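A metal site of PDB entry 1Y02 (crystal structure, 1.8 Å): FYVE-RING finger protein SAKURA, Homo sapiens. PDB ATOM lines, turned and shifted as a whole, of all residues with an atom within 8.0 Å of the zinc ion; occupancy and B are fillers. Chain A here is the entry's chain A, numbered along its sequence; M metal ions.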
ATOM      1  N   SER A  21      -1.916 -12.764   0.507  1.00  0.00           N
ATOM      2  CA  SER A  21      -1.720 -12.120   1.796  1.00  0.00           C
ATOM      3  C   SER A  21      -1.452 -13.171   2.872  1.00  0.00           C
ATOM      4  O   SER A  21      -1.648 -14.364   2.651  1.00  0.00           O
ATOM      5  CB  SER A  21      -2.956 -11.303   2.173  1.00  0.00           C
ATOM      6  OG  SER A  21      -4.103 -12.131   2.262  1.00  0.00           O
ATOM      7  N   CYS A  22      -0.993 -12.727   4.031  1.00  0.00           N
ATOM      8  CA  CYS A  22      -0.711 -13.650   5.121  1.00  0.00           C
ATOM      9  C   CYS A  22      -1.994 -14.190   5.733  1.00  0.00           C
ATOM     10  O   CYS A  22      -2.899 -13.431   6.101  1.00  0.00           O
ATOM     11  CB  CYS A  22       0.100 -12.963   6.225  1.00  0.00           C
ATOM     12  SG  CYS A  22       0.472 -14.035   7.609  1.00  0.00           S
ATOM     13  N   LYS A  23      -2.066 -15.514   5.843  1.00  0.00           N
ATOM     14  CA  LYS A  23      -3.237 -16.172   6.402  1.00  0.00           C
ATOM     15  C   LYS A  23      -3.446 -15.845   7.887  1.00  0.00           C
ATOM     16  O   LYS A  23      -4.563 -15.899   8.382  1.00  0.00           O
ATOM     17  CB  LYS A  23      -3.093 -17.687   6.198  1.00  0.00           C
ATOM     18  CG  LYS A  23      -4.260 -18.526   6.720  1.00  0.00           C
ATOM     19  CD  LYS A  23      -5.570 -18.230   5.996  1.00  0.00           C
ATOM     20  CE  LYS A  23      -5.523 -18.654   4.543  1.00  0.00           C
ATOM     21  NZ  LYS A  23      -6.806 -18.313   3.842  1.00  0.00           N
ATOM     22  N   SER A  24      -2.365 -15.508   8.582  1.00  0.00           N
ATOM     23  CA  SER A  24      -2.458 -15.200  10.000  1.00  0.00           C
ATOM     24  C   SER A  24      -2.822 -13.751  10.311  1.00  0.00           C
ATOM     25  O   SER A  24      -3.871 -13.478  10.899  1.00  0.00           O
ATOM     26  CB  SER A  24      -1.148 -15.564  10.705  1.00  0.00           C
ATOM     27  OG  SER A  24      -1.238 -15.332  12.108  1.00  0.00           O
ATOM     28  N   CYS A  25      -1.967 -12.818   9.904  1.00  0.00           N
ATOM     29  CA  CYS A  25      -2.186 -11.405  10.186  1.00  0.00           C
ATOM     30  C   CYS A  25      -2.903 -10.619   9.091  1.00  0.00           C
ATOM     31  O   CYS A  25      -3.313  -9.475   9.314  1.00  0.00           O
ATOM     32  CB  CYS A  25      -0.850 -10.719  10.524  1.00  0.00           C
ATOM     33  SG  CYS A  25       0.237 -10.492   9.119  1.00  0.00           S
ATOM     34  N   GLY A  26      -3.052 -11.223   7.920  1.00  0.00           N
ATOM     35  CA  GLY A  26      -3.731 -10.562   6.828  1.00  0.00           C
ATOM     36  C   GLY A  26      -2.920  -9.544   6.039  1.00  0.00           C
ATOM     37  O   GLY A  26      -3.409  -9.001   5.051  1.00  0.00           O
ATOM     38  N   ALA A  27      -1.692  -9.280   6.469  1.00  0.00           N
ATOM     39  CA  ALA A  27      -0.856  -8.310   5.775  1.00  0.00           C
ATOM     40  C   ALA A  27      -0.386  -8.813   4.418  1.00  0.00           C
ATOM     41  O   ALA A  27      -0.451 -10.014   4.118  1.00  0.00           O
ATOM     42  CB  ALA A  27       0.352  -7.949   6.644  1.00  0.00           C
ATOM     43  N   HIS A  28       0.079  -7.885   3.587  1.00  0.00           N
ATOM     44  CA  HIS A  28       0.589  -8.215   2.268  1.00  0.00           C
ATOM     45  C   HIS A  28       2.097  -8.361   2.348  1.00  0.00           C
ATOM     46  O   HIS A  28       2.701  -8.157   3.396  1.00  0.00           O
ATOM     47  CB  HIS A  28       0.214  -7.131   1.259  1.00  0.00           C
ATOM     48  CG  HIS A  28      -1.223  -7.168   0.837  1.00  0.00           C
ATOM     49  ND1 HIS A  28      -2.270  -7.092   1.730  1.00  0.00           N
ATOM     50  CD2 HIS A  28      -1.789  -7.308  -0.388  1.00  0.00           C
ATOM     51  CE1 HIS A  28      -3.408  -7.169   1.078  1.00  0.00           C
ATOM     52  NE2 HIS A  28      -3.149  -7.300  -0.214  1.00  0.00           N
ATOM     53  N   PHE A  29       2.706  -8.723   1.223  1.00  0.00           N
ATOM     54  CA  PHE A  29       4.156  -8.916   1.156  1.00  0.00           C
ATOM     55  C   PHE A  29       4.804  -7.857   0.277  1.00  0.00           C
ATOM     56  O   PHE A  29       4.281  -7.532  -0.797  1.00  0.00           O
ATOM     57  CB  PHE A  29       4.447 -10.307   0.589  1.00  0.00           C
ATOM     58  CG  PHE A  29       3.742 -11.426   1.317  1.00  0.00           C
ATOM     59  CD1 PHE A  29       4.215 -11.876   2.547  1.00  0.00           C
ATOM     60  CD2 PHE A  29       2.603 -12.006   0.780  1.00  0.00           C
ATOM     61  CE1 PHE A  29       3.544 -12.888   3.233  1.00  0.00           C
ATOM     62  CE2 PHE A  29       1.930 -13.023   1.458  1.00  0.00           C
ATOM     63  CZ  PHE A  29       2.400 -13.464   2.684  1.00  0.00           C
ATOM     64  N   ASN A  44      -0.214 -19.406   2.987  1.00  0.00           N
ATOM     65  CA  ASN A  44       0.903 -18.463   2.936  1.00  0.00           C
ATOM     66  C   ASN A  44       0.978 -17.560   4.169  1.00  0.00           C
ATOM     67  O   ASN A  44      -0.043 -17.115   4.664  1.00  0.00           O
ATOM     68  CB  ASN A  44       0.802 -17.593   1.667  1.00  0.00           C
ATOM     69  CG  ASN A  44       0.758 -18.421   0.400  1.00  0.00           C
ATOM     70  OD1 ASN A  44       1.528 -19.360   0.229  1.00  0.00           O
ATOM     71  ND2 ASN A  44      -0.154 -18.069  -0.502  1.00  0.00           N
ATOM     72  N   PHE A  45       2.202 -17.300   4.640  1.00  0.00           N
ATOM     73  CA  PHE A  45       2.407 -16.485   5.844  1.00  0.00           C
ATOM     74  C   PHE A  45       3.620 -15.576   5.779  1.00  0.00           C
ATOM     75  O   PHE A  45       4.514 -15.761   4.959  1.00  0.00           O
ATOM     76  CB  PHE A  45       2.620 -17.378   7.063  1.00  0.00           C
ATOM     77  CG  PHE A  45       1.524 -18.359   7.303  1.00  0.00           C
ATOM     78  CD1 PHE A  45       1.478 -19.562   6.615  1.00  0.00           C
ATOM     79  CD2 PHE A  45       0.541 -18.084   8.247  1.00  0.00           C
ATOM     80  CE1 PHE A  45       0.461 -20.483   6.852  1.00  0.00           C
ATOM     81  CE2 PHE A  45      -0.486 -18.993   8.491  1.00  0.00           C
ATOM     82  CZ  PHE A  45      -0.528 -20.190   7.787  1.00  0.00           C
ATOM     83  N   CYS A  46       3.647 -14.605   6.692  1.00  0.00           N
ATOM     84  CA  CYS A  46       4.773 -13.667   6.812  1.00  0.00           C
ATOM     85  C   CYS A  46       5.922 -14.469   7.381  1.00  0.00           C
ATOM     86  O   CYS A  46       5.723 -15.532   7.954  1.00  0.00           O
ATOM     87  CB  CYS A  46       4.480 -12.563   7.830  1.00  0.00           C
ATOM     88  SG  CYS A  46       3.167 -11.466   7.445  1.00  0.00           S
ATOM     89  N   MET A  47       7.130 -13.932   7.229  1.00  0.00           N
ATOM     90  CA  MET A  47       8.301 -14.578   7.791  1.00  0.00           C
ATOM     91  C   MET A  47       8.111 -14.487   9.305  1.00  0.00           C
ATOM     92  O   MET A  47       8.493 -15.374  10.053  1.00  0.00           O
ATOM     93  CB  MET A  47       9.556 -13.834   7.371  1.00  0.00           C
ATOM     94  CG  MET A  47      10.846 -14.439   7.889  1.00  0.00           C
ATOM     95  SD  MET A  47      11.192 -16.044   7.139  1.00  0.00           S
ATOM     96  CE  MET A  47      11.773 -15.543   5.523  1.00  0.00           C
ATOM     97  N   THR A  48       7.482 -13.389   9.745  1.00  0.00           N
ATOM     98  CA  THR A  48       7.237 -13.163  11.169  1.00  0.00           C
ATOM     99  C   THR A  48       6.029 -13.922  11.693  1.00  0.00           C
ATOM    100  O   THR A  48       5.697 -13.847  12.874  1.00  0.00           O
ATOM    101  CB  THR A  48       7.067 -11.658  11.487  1.00  0.00           C
ATOM    102  OG1 THR A  48       6.118 -11.086  10.584  1.00  0.00           O
ATOM    103  CG2 THR A  48       8.397 -10.938  11.363  1.00  0.00           C
ATOM    104  N   CYS A  49       5.367 -14.652  10.797  1.00  0.00           N
ATOM    105  CA  CYS A  49       4.206 -15.449  11.191  1.00  0.00           C
ATOM    106  C   CYS A  49       4.472 -16.931  10.948  1.00  0.00           C
ATOM    107  O   CYS A  49       3.550 -17.731  10.828  1.00  0.00           O
ATOM    108  CB  CYS A  49       2.958 -15.001  10.424  1.00  0.00           C
ATOM    109  SG  CYS A  49       2.355 -13.367  10.915  1.00  0.00           S
ATOM    110  N   SER A  50       5.752 -17.276  10.852  1.00  0.00           N
ATOM    111  CA  SER A  50       6.172 -18.657  10.638  1.00  0.00           C
ATOM    112  C   SER A  50       7.508 -18.860  11.345  1.00  0.00           C
ATOM    113  O   SER A  50       8.098 -17.904  11.831  1.00  0.00           O
ATOM    114  CB  SER A  50       6.294 -18.950   9.139  1.00  0.00           C
ATOM    115  OG  SER A  50       7.168 -18.052   8.488  1.00  0.00           O
HETATM  116 ZN    ZN M   1       1.605 -12.411   8.901  1.00  0.00          ZN
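The backbone carbonyl oxygen (O) of Cys 46 is in hydrogen-bond range of the side-chain hydroxyl (OG) of Ser 50 (3.0 Å).
The backbone NH (N) of Ser 24 sits close to the side-chain sulfur (SG) of Cys 22, at 3.3 Å.
O of Ala 27 is in hydrogen-bond range of N of Cys 22.
The side-chain sulfur (SG) of Cys 25 sits close to the backbone NH (N) of Ala 27.
Within 4 Å of the zinc ion: Cys 22, Cys 25, Cys 46 and Cys 49.
The zinc ion is bound by the side-chain sulfur (SG) of Cys 46 (2.3 Å), the side-chain sulfur (SG) of Cys 49 (2.4 Å), the side-chain sulfur (SG) of Cys 22 (2.4 Å) and the side-chain sulfur (SG) of Cys 25 (2.4 Å).
The zinc ion has four donor atoms within binding distance.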
